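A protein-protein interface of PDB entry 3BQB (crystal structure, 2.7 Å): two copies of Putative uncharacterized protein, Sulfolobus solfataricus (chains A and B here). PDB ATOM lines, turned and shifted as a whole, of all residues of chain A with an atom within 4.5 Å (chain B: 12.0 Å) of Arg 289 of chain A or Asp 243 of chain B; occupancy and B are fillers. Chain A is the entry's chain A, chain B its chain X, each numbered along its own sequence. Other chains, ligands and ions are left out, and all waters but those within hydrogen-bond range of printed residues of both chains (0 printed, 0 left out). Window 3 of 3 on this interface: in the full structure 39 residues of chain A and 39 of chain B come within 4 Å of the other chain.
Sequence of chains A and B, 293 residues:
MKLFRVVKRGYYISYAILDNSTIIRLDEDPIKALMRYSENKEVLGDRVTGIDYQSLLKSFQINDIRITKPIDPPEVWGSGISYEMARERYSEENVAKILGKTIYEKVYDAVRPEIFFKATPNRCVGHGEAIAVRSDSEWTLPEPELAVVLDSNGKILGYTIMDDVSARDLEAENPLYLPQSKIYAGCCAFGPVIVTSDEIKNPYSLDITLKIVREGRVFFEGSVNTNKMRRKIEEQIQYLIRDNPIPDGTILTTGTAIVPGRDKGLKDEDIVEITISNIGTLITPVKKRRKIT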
ATOM      1  N   ALA A 132      16.653 -37.865 -11.855  1.00  0.00           N
ATOM      2  CA  ALA A 132      15.407 -37.998 -12.616  1.00  0.00           C
ATOM      3  C   ALA A 132      15.598 -37.923 -14.123  1.00  0.00           C
ATOM      4  O   ALA A 132      16.541 -37.293 -14.615  1.00  0.00           O
ATOM      5  CB  ALA A 132      14.412 -36.943 -12.184  1.00  0.00           C
ATOM      6  N   VAL A 133      14.689 -38.584 -14.837  1.00  0.00           N
ATOM      7  CA  VAL A 133      14.504 -38.397 -16.269  1.00  0.00           C
ATOM      8  C   VAL A 133      13.176 -37.668 -16.456  1.00  0.00           C
ATOM      9  O   VAL A 133      12.146 -38.105 -15.937  1.00  0.00           O
ATOM     10  CB  VAL A 133      14.453 -39.754 -17.020  1.00  0.00           C
ATOM     11  CG1 VAL A 133      14.032 -39.561 -18.484  1.00  0.00           C
ATOM     12  CG2 VAL A 133      15.799 -40.468 -16.935  1.00  0.00           C
ATOM     13  N   ARG A 134      13.196 -36.570 -17.205  1.00  0.00           N
ATOM     14  CA  ARG A 134      11.988 -35.784 -17.436  1.00  0.00           C
ATOM     15  C   ARG A 134      10.917 -36.627 -18.113  1.00  0.00           C
ATOM     16  O   ARG A 134      11.227 -37.494 -18.927  1.00  0.00           O
ATOM     17  CB  ARG A 134      12.287 -34.567 -18.311  1.00  0.00           C
ATOM     18  CG  ARG A 134      13.200 -33.525 -17.682  1.00  0.00           C
ATOM     19  CD  ARG A 134      13.566 -32.454 -18.697  1.00  0.00           C
ATOM     20  NE  ARG A 134      12.368 -31.862 -19.297  1.00  0.00           N
ATOM     21  CZ  ARG A 134      11.823 -30.697 -18.945  1.00  0.00           C
ATOM     22  NH1 ARG A 134      12.374 -29.931 -18.014  1.00  0.00           N
ATOM     23  NH2 ARG A 134      10.719 -30.285 -19.552  1.00  0.00           N
ATOM     24  N   SER A 135       9.658 -36.362 -17.780  1.00  0.00           N
ATOM     25  CA  SER A 135       8.533 -37.074 -18.382  1.00  0.00           C
ATOM     26  C   SER A 135       8.523 -36.997 -19.922  1.00  0.00           C
ATOM     27  O   SER A 135       8.095 -37.934 -20.589  1.00  0.00           O
ATOM     28  CB  SER A 135       7.203 -36.550 -17.823  1.00  0.00           C
ATOM     29  OG  SER A 135       6.981 -35.198 -18.190  1.00  0.00           O
ATOM     30  N   ASP A 136       9.015 -35.890 -20.472  1.00  0.00           N
ATOM     31  CA  ASP A 136       8.940 -35.635 -21.909  1.00  0.00           C
ATOM     32  C   ASP A 136      10.253 -35.932 -22.650  1.00  0.00           C
ATOM     33  O   ASP A 136      10.404 -35.550 -23.814  1.00  0.00           O
ATOM     34  CB  ASP A 136       8.503 -34.183 -22.152  1.00  0.00           C
ATOM     35  CG  ASP A 136       9.417 -33.160 -21.469  1.00  0.00           C
ATOM     36  OD1 ASP A 136       9.170 -31.949 -21.622  1.00  0.00           O
ATOM     37  OD2 ASP A 136      10.375 -33.558 -20.777  1.00  0.00           O
ATOM     38  N   TYR A 184      15.828 -29.156 -13.861  1.00  0.00           N
ATOM     39  CA  TYR A 184      14.559 -29.727 -13.420  1.00  0.00           C
ATOM     40  C   TYR A 184      14.790 -30.477 -12.113  1.00  0.00           C
ATOM     41  O   TYR A 184      15.912 -30.520 -11.615  1.00  0.00           O
ATOM     42  CB  TYR A 184      13.977 -30.645 -14.502  1.00  0.00           C
ATOM     43  CG  TYR A 184      14.915 -31.729 -14.968  1.00  0.00           C
ATOM     44  CD1 TYR A 184      14.831 -33.012 -14.449  1.00  0.00           C
ATOM     45  CD2 TYR A 184      15.888 -31.476 -15.933  1.00  0.00           C
ATOM     46  CE1 TYR A 184      15.688 -34.018 -14.869  1.00  0.00           C
ATOM     47  CE2 TYR A 184      16.752 -32.480 -16.362  1.00  0.00           C
ATOM     48  CZ  TYR A 184      16.644 -33.749 -15.823  1.00  0.00           C
ATOM     49  OH  TYR A 184      17.485 -34.753 -16.231  1.00  0.00           O
ATOM     50  N   ALA A 185      13.738 -31.050 -11.541  1.00  0.00           N
ATOM     51  CA  ALA A 185      13.875 -31.767 -10.270  1.00  0.00           C
ATOM     52  C   ALA A 185      14.731 -33.022 -10.455  1.00  0.00           C
ATOM     53  O   ALA A 185      14.387 -33.895 -11.249  1.00  0.00           O
ATOM     54  CB  ALA A 185      12.499 -32.126  -9.695  1.00  0.00           C
ATOM     55  N   LYS A 287      14.865 -42.216 -11.455  1.00  0.00           N
ATOM     56  CA  LYS A 287      13.417 -42.165 -11.460  1.00  0.00           C
ATOM     57  C   LYS A 287      12.955 -41.504 -12.759  1.00  0.00           C
ATOM     58  O   LYS A 287      13.492 -40.475 -13.159  1.00  0.00           O
ATOM     59  CB  LYS A 287      12.923 -41.397 -10.229  1.00  0.00           C
ATOM     60  CG  LYS A 287      11.418 -41.090 -10.196  1.00  0.00           C
ATOM     61  CD  LYS A 287      10.556 -42.352 -10.264  1.00  0.00           C
ATOM     62  CE  LYS A 287       9.065 -42.023 -10.210  1.00  0.00           C
ATOM     63  NZ  LYS A 287       8.224 -43.239 -10.437  1.00  0.00           N
ATOM     64  N   LYS A 288      11.982 -42.120 -13.426  1.00  0.00           N
ATOM     65  CA  LYS A 288      11.355 -41.543 -14.618  1.00  0.00           C
ATOM     66  C   LYS A 288      10.042 -40.877 -14.207  1.00  0.00           C
ATOM     67  O   LYS A 288       9.186 -41.506 -13.587  1.00  0.00           O
ATOM     68  CB  LYS A 288      11.106 -42.631 -15.674  1.00  0.00           C
ATOM     69  CG  LYS A 288      10.220 -42.226 -16.859  1.00  0.00           C
ATOM     70  CD  LYS A 288      10.908 -41.255 -17.807  1.00  0.00           C
ATOM     71  CE  LYS A 288      10.036 -40.987 -19.032  1.00  0.00           C
ATOM     72  NZ  LYS A 288      10.648 -40.041 -20.006  1.00  0.00           N
ATOM     73  N   ARG A 289       9.888 -39.607 -14.565  1.00  0.00           N
ATOM     74  CA  ARG A 289       8.717 -38.834 -14.163  1.00  0.00           C
ATOM     75  C   ARG A 289       7.499 -39.218 -14.995  1.00  0.00           C
ATOM     76  O   ARG A 289       7.613 -39.494 -16.187  1.00  0.00           O
ATOM     77  CB  ARG A 289       8.992 -37.334 -14.305  1.00  0.00           C
ATOM     78  CG  ARG A 289      10.191 -36.823 -13.509  1.00  0.00           C
ATOM     79  CD  ARG A 289       9.976 -36.955 -12.016  1.00  0.00           C
ATOM     80  NE  ARG A 289      11.114 -36.433 -11.266  1.00  0.00           N
ATOM     81  CZ  ARG A 289      11.245 -36.503  -9.942  1.00  0.00           C
ATOM     82  NH1 ARG A 289      12.332 -35.997  -9.367  1.00  0.00           N
ATOM     83  NH2 ARG A 289      10.304 -37.075  -9.189  1.00  0.00           N
ATOM     84  N   ARG A 290       6.336 -39.222 -14.352  1.00  0.00           N
ATOM     85  CA  ARG A 290       5.074 -39.592 -14.989  1.00  0.00           C
ATOM     86  C   ARG A 290       4.406 -38.328 -15.563  1.00  0.00           C
ATOM     87  O   ARG A 290       4.933 -37.225 -15.409  1.00  0.00           O
ATOM     88  CB  ARG A 290       4.179 -40.282 -13.952  1.00  0.00           C
ATOM     89  CG  ARG A 290       3.128 -41.232 -14.518  1.00  0.00           C
ATOM     90  CD  ARG A 290       2.354 -41.938 -13.401  1.00  0.00           C
ATOM     91  NE  ARG A 290       0.906 -41.739 -13.538  1.00  0.00           N
ATOM     92  CZ  ARG A 290       0.100 -42.428 -14.351  1.00  0.00           C
ATOM     93  NH1 ARG A 290       0.575 -43.399 -15.135  1.00  0.00           N
ATOM     94  NH2 ARG A 290      -1.202 -42.142 -14.382  1.00  0.00           N
ATOM     95  N   LYS A 291       3.271 -38.493 -16.244  1.00  0.00           N
ATOM     96  CA  LYS A 291       2.501 -37.364 -16.785  1.00  0.00           C
ATOM     97  C   LYS A 291       1.105 -37.318 -16.171  1.00  0.00           C
ATOM     98  O   LYS A 291       0.631 -36.257 -15.765  1.00  0.00           O
ATOM     99  CB  LYS A 291       2.404 -37.473 -18.309  1.00  0.00           C
ATOM    100  CG  LYS A 291       3.755 -37.417 -19.007  1.00  0.00           C
ATOM    101  CD  LYS A 291       3.682 -37.834 -20.478  1.00  0.00           C
ATOM    102  CE  LYS A 291       5.088 -37.991 -21.062  1.00  0.00           C
ATOM    103  NZ  LYS A 291       5.112 -38.435 -22.485  1.00  0.00           N
ATOM    104  N   GLU B  75      13.312 -17.164  -7.888  1.00  0.00           N
ATOM    105  CA  GLU B  75      13.807 -17.466  -9.231  1.00  0.00           C
ATOM    106  C   GLU B  75      13.113 -16.582 -10.263  1.00  0.00           C
ATOM    107  O   GLU B  75      11.976 -16.164 -10.067  1.00  0.00           O
ATOM    108  CB  GLU B  75      13.576 -18.941  -9.568  1.00  0.00           C
ATOM    109  CG  GLU B  75      14.320 -19.909  -8.649  1.00  0.00           C
ATOM    110  CD  GLU B  75      13.878 -21.346  -8.811  1.00  0.00           C
ATOM    111  OE1 GLU B  75      13.159 -21.647  -9.778  1.00  0.00           O
ATOM    112  OE2 GLU B  75      14.252 -22.170  -7.956  1.00  0.00           O
ATOM    113  N   TRP B  77      12.476 -16.676 -14.499  1.00  0.00           N
ATOM    114  CA  TRP B  77      12.598 -17.343 -15.790  1.00  0.00           C
ATOM    115  C   TRP B  77      12.012 -16.462 -16.885  1.00  0.00           C
ATOM    116  O   TRP B  77      11.263 -15.527 -16.610  1.00  0.00           O
ATOM    117  CB  TRP B  77      11.877 -18.695 -15.763  1.00  0.00           C
ATOM    118  CG  TRP B  77      12.448 -19.663 -14.762  1.00  0.00           C
ATOM    119  CD1 TRP B  77      12.413 -19.553 -13.403  1.00  0.00           C
ATOM    120  CD2 TRP B  77      13.129 -20.889 -15.044  1.00  0.00           C
ATOM    121  NE1 TRP B  77      13.030 -20.626 -12.825  1.00  0.00           N
ATOM    122  CE2 TRP B  77      13.479 -21.466 -13.809  1.00  0.00           C
ATOM    123  CE3 TRP B  77      13.473 -21.560 -16.223  1.00  0.00           C
ATOM    124  CZ2 TRP B  77      14.160 -22.677 -13.715  1.00  0.00           C
ATOM    125  CZ3 TRP B  77      14.150 -22.761 -16.129  1.00  0.00           C
ATOM    126  CH2 TRP B  77      14.487 -23.308 -14.882  1.00  0.00           C
ATOM    127  N   ARG B 112       7.010 -27.097 -28.357  1.00  0.00           N
ATOM    128  CA  ARG B 112       7.775 -26.691 -27.190  1.00  0.00           C
ATOM    129  C   ARG B 112       8.267 -25.265 -27.378  1.00  0.00           C
ATOM    130  O   ARG B 112       8.917 -24.977 -28.380  1.00  0.00           O
ATOM    131  CB  ARG B 112       8.978 -27.613 -26.985  1.00  0.00           C
ATOM    132  CG  ARG B 112       9.817 -27.264 -25.759  1.00  0.00           C
ATOM    133  CD  ARG B 112      10.971 -28.230 -25.549  1.00  0.00           C
ATOM    134  NE  ARG B 112      10.544 -29.629 -25.542  1.00  0.00           N
ATOM    135  CZ  ARG B 112       9.866 -30.224 -24.561  1.00  0.00           C
ATOM    136  NH1 ARG B 112       9.541 -31.505 -24.679  1.00  0.00           N
ATOM    137  NH2 ARG B 112       9.508 -29.557 -23.470  1.00  0.00           N
ATOM    138  N   ILE B 115      12.136 -21.699 -22.923  1.00  0.00           N
ATOM    139  CA  ILE B 115      12.096 -21.334 -21.509  1.00  0.00           C
ATOM    140  C   ILE B 115      13.520 -21.343 -20.980  1.00  0.00           C
ATOM    141  O   ILE B 115      14.217 -22.346 -21.107  1.00  0.00           O
ATOM    142  CB  ILE B 115      11.273 -22.334 -20.686  1.00  0.00           C
ATOM    143  CG1 ILE B 115       9.813 -22.361 -21.155  1.00  0.00           C
ATOM    144  CG2 ILE B 115      11.355 -21.998 -19.196  1.00  0.00           C
ATOM    145  CD1 ILE B 115       9.023 -21.091 -20.845  1.00  0.00           C
ATOM    146  N   SER B 152       3.877 -22.007  -6.525  1.00  0.00           N
ATOM    147  CA  SER B 152       4.519 -23.267  -6.920  1.00  0.00           C
ATOM    148  C   SER B 152       3.660 -24.113  -7.861  1.00  0.00           C
ATOM    149  O   SER B 152       4.195 -24.930  -8.600  1.00  0.00           O
ATOM    150  CB  SER B 152       4.929 -24.085  -5.695  1.00  0.00           C
ATOM    151  OG  SER B 152       3.824 -24.320  -4.849  1.00  0.00           O
ATOM    152  N   ASN B 153       2.345 -23.903  -7.841  1.00  0.00           N
ATOM    153  CA  ASN B 153       1.416 -24.604  -8.738  1.00  0.00           C
ATOM    154  C   ASN B 153       1.268 -23.967 -10.124  1.00  0.00           C
ATOM    155  O   ASN B 153       0.532 -24.489 -10.971  1.00  0.00           O
ATOM    156  CB  ASN B 153       0.029 -24.697  -8.097  1.00  0.00           C
ATOM    157  CG  ASN B 153       0.029 -25.506  -6.819  1.00  0.00           C
ATOM    158  OD1 ASN B 153       0.892 -26.358  -6.608  1.00  0.00           O
ATOM    159  ND2 ASN B 153      -0.947 -25.242  -5.954  1.00  0.00           N
ATOM    160  N   GLY B 154       1.951 -22.843 -10.350  1.00  0.00           N
ATOM    161  CA  GLY B 154       1.867 -22.124 -11.620  1.00  0.00           C
ATOM    162  C   GLY B 154       0.737 -21.110 -11.698  1.00  0.00           C
ATOM    163  O   GLY B 154       0.533 -20.487 -12.736  1.00  0.00           O
ATOM    164  N   GLU B 235       0.480 -21.557 -21.584  1.00  0.00           N
ATOM    165  CA  GLU B 235       1.400 -22.518 -22.181  1.00  0.00           C
ATOM    166  C   GLU B 235       2.818 -22.323 -21.648  1.00  0.00           C
ATOM    167  O   GLU B 235       3.490 -23.292 -21.297  1.00  0.00           O
ATOM    168  CB  GLU B 235       1.402 -22.396 -23.708  1.00  0.00           C
ATOM    169  CG  GLU B 235       2.141 -23.531 -24.410  1.00  0.00           C
ATOM    170  CD  GLU B 235       2.203 -23.366 -25.913  1.00  0.00           C
ATOM    171  OE1 GLU B 235       2.361 -24.389 -26.612  1.00  0.00           O
ATOM    172  OE2 GLU B 235       2.087 -22.224 -26.403  1.00  0.00           O
ATOM    173  N   GLN B 236       3.268 -21.072 -21.586  1.00  0.00           N
ATOM    174  CA  GLN B 236       4.598 -20.759 -21.055  1.00  0.00           C
ATOM    175  C   GLN B 236       4.790 -21.337 -19.647  1.00  0.00           C
ATOM    176  O   GLN B 236       5.842 -21.910 -19.348  1.00  0.00           O
ATOM    177  CB  GLN B 236       4.844 -19.249 -21.029  1.00  0.00           C
ATOM    178  CG  GLN B 236       4.775 -18.568 -22.391  1.00  0.00           C
ATOM    179  CD  GLN B 236       5.219 -17.118 -22.350  1.00  0.00           C
ATOM    180  OE1 GLN B 236       5.802 -16.662 -21.372  1.00  0.00           O
ATOM    181  NE2 GLN B 236       4.954 -16.388 -23.423  1.00  0.00           N
ATOM    182  N   ILE B 237       3.769 -21.192 -18.801  1.00  0.00           N
ATOM    183  CA  ILE B 237       3.803 -21.717 -17.434  1.00  0.00           C
ATOM    184  C   ILE B 237       3.805 -23.242 -17.428  1.00  0.00           C
ATOM    185  O   ILE B 237       4.555 -23.853 -16.673  1.00  0.00           O
ATOM    186  CB  ILE B 237       2.608 -21.200 -16.580  1.00  0.00           C
ATOM    187  CG1 ILE B 237       2.705 -19.682 -16.377  1.00  0.00           C
ATOM    188  CG2 ILE B 237       2.576 -21.877 -15.216  1.00  0.00           C
ATOM    189  CD1 ILE B 237       1.413 -19.027 -15.882  1.00  0.00           C
ATOM    190  N   GLN B 238       2.961 -23.850 -18.260  1.00  0.00           N
ATOM    191  CA  GLN B 238       2.888 -25.315 -18.361  1.00  0.00           C
ATOM    192  C   GLN B 238       4.275 -25.924 -18.590  1.00  0.00           C
ATOM    193  O   GLN B 238       4.663 -26.880 -17.914  1.00  0.00           O
ATOM    194  CB  GLN B 238       1.949 -25.735 -19.498  1.00  0.00           C
ATOM    195  CG  GLN B 238       1.589 -27.231 -19.508  1.00  0.00           C
ATOM    196  CD  GLN B 238       1.305 -27.793 -20.912  1.00  0.00           C
ATOM    197  OE1 GLN B 238       1.376 -27.082 -21.918  1.00  0.00           O
ATOM    198  NE2 GLN B 238       0.991 -29.080 -20.972  1.00  0.00           N
ATOM    199  N   TYR B 239       5.021 -25.359 -19.536  1.00  0.00           N
ATOM    200  CA  TYR B 239       6.363 -25.851 -19.839  1.00  0.00           C
ATOM    201  C   TYR B 239       7.389 -25.472 -18.776  1.00  0.00           C
ATOM    202  O   TYR B 239       8.341 -26.214 -18.550  1.00  0.00           O
ATOM    203  CB  TYR B 239       6.814 -25.398 -21.238  1.00  0.00           C
ATOM    204  CG  TYR B 239       6.204 -26.252 -22.326  1.00  0.00           C
ATOM    205  CD1 TYR B 239       4.989 -25.906 -22.913  1.00  0.00           C
ATOM    206  CD2 TYR B 239       6.821 -27.431 -22.739  1.00  0.00           C
ATOM    207  CE1 TYR B 239       4.415 -26.699 -23.897  1.00  0.00           C
ATOM    208  CE2 TYR B 239       6.255 -28.232 -23.721  1.00  0.00           C
ATOM    209  CZ  TYR B 239       5.052 -27.860 -24.294  1.00  0.00           C
ATOM    210  OH  TYR B 239       4.489 -28.648 -25.264  1.00  0.00           O
ATOM    211  N   LEU B 240       7.194 -24.330 -18.121  1.00  0.00           N
ATOM    212  CA  LEU B 240       8.081 -23.905 -17.033  1.00  0.00           C
ATOM    213  C   LEU B 240       8.091 -24.903 -15.884  1.00  0.00           C
ATOM    214  O   LEU B 240       9.150 -25.265 -15.387  1.00  0.00           O
ATOM    215  CB  LEU B 240       7.677 -22.522 -16.502  1.00  0.00           C
ATOM    216  CG  LEU B 240       8.391 -21.996 -15.246  1.00  0.00           C
ATOM    217  CD1 LEU B 240       9.904 -21.980 -15.416  1.00  0.00           C
ATOM    218  CD2 LEU B 240       7.892 -20.604 -14.891  1.00  0.00           C
ATOM    219  N   ILE B 241       6.908 -25.342 -15.469  1.00  0.00           N
ATOM    220  CA  ILE B 241       6.776 -26.115 -14.241  1.00  0.00           C
ATOM    221  C   ILE B 241       6.838 -27.624 -14.450  1.00  0.00           C
ATOM    222  O   ILE B 241       6.936 -28.372 -13.481  1.00  0.00           O
ATOM    223  CB  ILE B 241       5.483 -25.741 -13.459  1.00  0.00           C
ATOM    224  CG1 ILE B 241       4.216 -26.090 -14.249  1.00  0.00           C
ATOM    225  CG2 ILE B 241       5.492 -24.264 -13.112  1.00  0.00           C
ATOM    226  CD1 ILE B 241       2.953 -25.976 -13.438  1.00  0.00           C
ATOM    227  N   ARG B 242       6.782 -28.064 -15.708  1.00  0.00           N
ATOM    228  CA  ARG B 242       6.857 -29.494 -16.046  1.00  0.00           C
ATOM    229  C   ARG B 242       8.124 -30.136 -15.484  1.00  0.00           C
ATOM    230  O   ARG B 242       9.231 -29.776 -15.892  1.00  0.00           O
ATOM    231  CB  ARG B 242       6.819 -29.691 -17.565  1.00  0.00           C
ATOM    232  CG  ARG B 242       7.125 -31.121 -18.021  1.00  0.00           C
ATOM    233  CD  ARG B 242       6.984 -31.267 -19.524  1.00  0.00           C
ATOM    234  NE  ARG B 242       5.592 -31.166 -19.951  1.00  0.00           N
ATOM    235  CZ  ARG B 242       5.182 -31.100 -21.215  1.00  0.00           C
ATOM    236  NH1 ARG B 242       6.054 -31.108 -22.220  1.00  0.00           N
ATOM    237  NH2 ARG B 242       3.882 -31.017 -21.474  1.00  0.00           N
ATOM    238  N   ASP B 243       7.950 -31.074 -14.546  1.00  0.00           N
ATOM    239  CA  ASP B 243       9.065 -31.766 -13.876  1.00  0.00           C
ATOM    240  C   ASP B 243      10.049 -30.797 -13.206  1.00  0.00           C
ATOM    241  O   ASP B 243      11.164 -31.180 -12.842  1.00  0.00           O
ATOM    242  CB  ASP B 243       9.815 -32.669 -14.870  1.00  0.00           C
ATOM    243  CG  ASP B 243       8.890 -33.611 -15.625  1.00  0.00           C
ATOM    244  OD1 ASP B 243       9.072 -33.761 -16.852  1.00  0.00           O
ATOM    245  OD2 ASP B 243       7.982 -34.203 -15.002  1.00  0.00           O
ATOM    246  N   ASN B 244       9.615 -29.555 -13.018  1.00  0.00           N
ATOM    247  CA  ASN B 244      10.489 -28.473 -12.595  1.00  0.00           C
ATOM    248  C   ASN B 244       9.768 -27.629 -11.550  1.00  0.00           C
ATOM    249  O   ASN B 244       9.093 -26.656 -11.886  1.00  0.00           O
ATOM    250  CB  ASN B 244      10.884 -27.627 -13.804  1.00  0.00           C
ATOM    251  CG  ASN B 244      11.863 -26.533 -13.457  1.00  0.00           C
ATOM    252  OD1 ASN B 244      12.729 -26.712 -12.604  1.00  0.00           O
ATOM    253  ND2 ASN B 244      11.741 -25.392 -14.128  1.00  0.00           N
ATOM    254  N   PRO B 245       9.915 -27.997 -10.271  1.00  0.00           N
ATOM    255  CA  PRO B 245       9.146 -27.331  -9.235  1.00  0.00           C
ATOM    256  C   PRO B 245       9.715 -25.945  -9.006  1.00  0.00           C
ATOM    257  O   PRO B 245      10.935 -25.784  -8.949  1.00  0.00           O
ATOM    258  CB  PRO B 245       9.368 -28.218  -8.009  1.00  0.00           C
ATOM    259  CG  PRO B 245      10.720 -28.815  -8.230  1.00  0.00           C
ATOM    260  CD  PRO B 245      10.844 -28.999  -9.718  1.00  0.00           C
ATOM    261  N   ILE B 246       8.837 -24.953  -8.906  1.00  0.00           N
ATOM    262  CA  ILE B 246       9.257 -23.577  -8.720  1.00  0.00           C
ATOM    263  C   ILE B 246       8.799 -23.098  -7.349  1.00  0.00           C
ATOM    264  O   ILE B 246       7.761 -23.529  -6.856  1.00  0.00           O
ATOM    265  CB  ILE B 246       8.706 -22.636  -9.832  1.00  0.00           C
ATOM    266  CG1 ILE B 246       7.190 -22.777  -9.991  1.00  0.00           C
ATOM    267  CG2 ILE B 246       9.393 -22.917 -11.166  1.00  0.00           C
ATOM    268  CD1 ILE B 246       6.572 -21.658 -10.781  1.00  0.00           C
ATOM    269  N   PRO B 247       9.589 -22.227  -6.713  1.00  0.00           N
ATOM    270  CA  PRO B 247       9.169 -21.625  -5.451  1.00  0.00           C
ATOM    271  C   PRO B 247       8.071 -20.559  -5.606  1.00  0.00           C
ATOM    272  O   PRO B 247       7.919 -19.954  -6.677  1.00  0.00           O
ATOM    273  CB  PRO B 247      10.460 -21.000  -4.919  1.00  0.00           C
ATOM    274  CG  PRO B 247      11.281 -20.735  -6.122  1.00  0.00           C
ATOM    275  CD  PRO B 247      10.936 -21.786  -7.122  1.00  0.00           C
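Hydrophobic or aromatic side chains of chain A within 4 Å of the printed part of chain B: Tyr 184 and Ala 185. Among the printed residues, 10 pairs touch across the chains.
N of Arg 289 of chain A lies within hydrogen-bond range of O of Val 133 of chain A (3.0 Å). The guanidinium group (NE) of Arg 134 of chain A is in salt-bridge range of the side-chain carboxylate (OD2) of Asp 136 of chain A, at 3.0 Å. O of Arg 134 of chain A lies within hydrogen-bond range of NZ of Lys 288 of chain A, 2.8 Å away. The side-chain amino group (NZ) of Lys 288 of chain A sits at hydrogen-bond distance from the backbone carbonyl oxygen (O) of Ser 135 of chain A, 3.4 Å away. O of Ala 185 of chain A sits at hydrogen-bond distance from NH1 of Arg 289 of chain A (3.5 Å). ND2 of Asn 244 of chain B is in hydrogen-bond range of O of Leu 240 of chain B, at 2.9 Å.
Arg 242 of chain B touches Arg 134 of chain A (O to NH1, 3.8 Å). Arg 134 of chain A touches Asp 243 of chain B (CA to OD1, 3.6 Å). Asp 243 of chain B touches Tyr 184 of chain A. Asn 244 of chain B touches Tyr 184 of chain A. Ala 185 of chain A touches Pro 245 of chain B. CB of Arg 289 of chain A touches OD2 of Asp 243 of chain B, 3.4 Å away.
No position is printed for both chains. Of the 10 pairs that touch across the chains among the printed residues, none has its exchanged pair printed and touching as well.
Arg 289 of chain A touches just one residue of chain B: Asp 243 (3.4 Å). Of the printed residues of chain A, Asp 243 of chain B touches Arg 134, Ser 135, Tyr 184, Ala 185 and Arg 289. No residue of chain B comes within 4 Å of Ala 132 of chain A. No residue of chain B comes within 4 Å of Val 133 of chain A. Of chain B, only Arg 242 (3.8 Å) and Asp 243 (3.6 Å) come within 4 Å of Arg 134 of chain A. Of chain B, only Asp 243 (2.8 Å) comes within 4 Å of Ser 135 of chain A. Ala 185 of chain A touches just these residues of chain B: Asp 243 (2.9 Å) and Pro 245 (3.5 Å). No residue of chain B comes within 4 Å of Lys 287 of chain A. No residue of chain B comes within 4 Å of Lys 291 of chain A. Of the printed residues of chain A, Asn 244 of chain B touches Tyr 184. Of the printed residues of chain A, Arg 112 of chain B touches Asp 136. Printed residues of chain A within 4 Å of Pro 245 of chain B: Ala 185 (3.5 Å). Printed residues of chain A within 4 Å of Arg 242 of chain B: Arg 134 (3.8 Å) and Asp 136 (3.1 Å). Asn 153 of chain B touches none of the printed residues of chain A. The nearest residue of chain B that does not touch Arg 289 of chain A is Pro 245 of chain B (7.2 Å). The nearest residue of chain A that does not touch Asp 243 of chain B is Asp 136 of chain A (4.1 Å). The nearest printed residue of chain A that does not touch Arg 112 of chain B is Arg 134 of chain A (4.2 Å).
N of Ser 135 of chain A sits at hydrogen-bond distance from OD1 of Asp 243 of chain B (2.8 Å). OD1 of Asp 136 of chain A is in salt-bridge range of NH2 of Arg 112 of chain B (3.0 Å). The guanidinium group (NH1) of Arg 242 of chain B is in salt-bridge range of the side-chain carboxylate (OD1) of Asp 136 of chain A (3.3 Å). N of Ala 185 of chain A lies within hydrogen-bond range of O of Asp 243 of chain B, at 2.9 Å.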
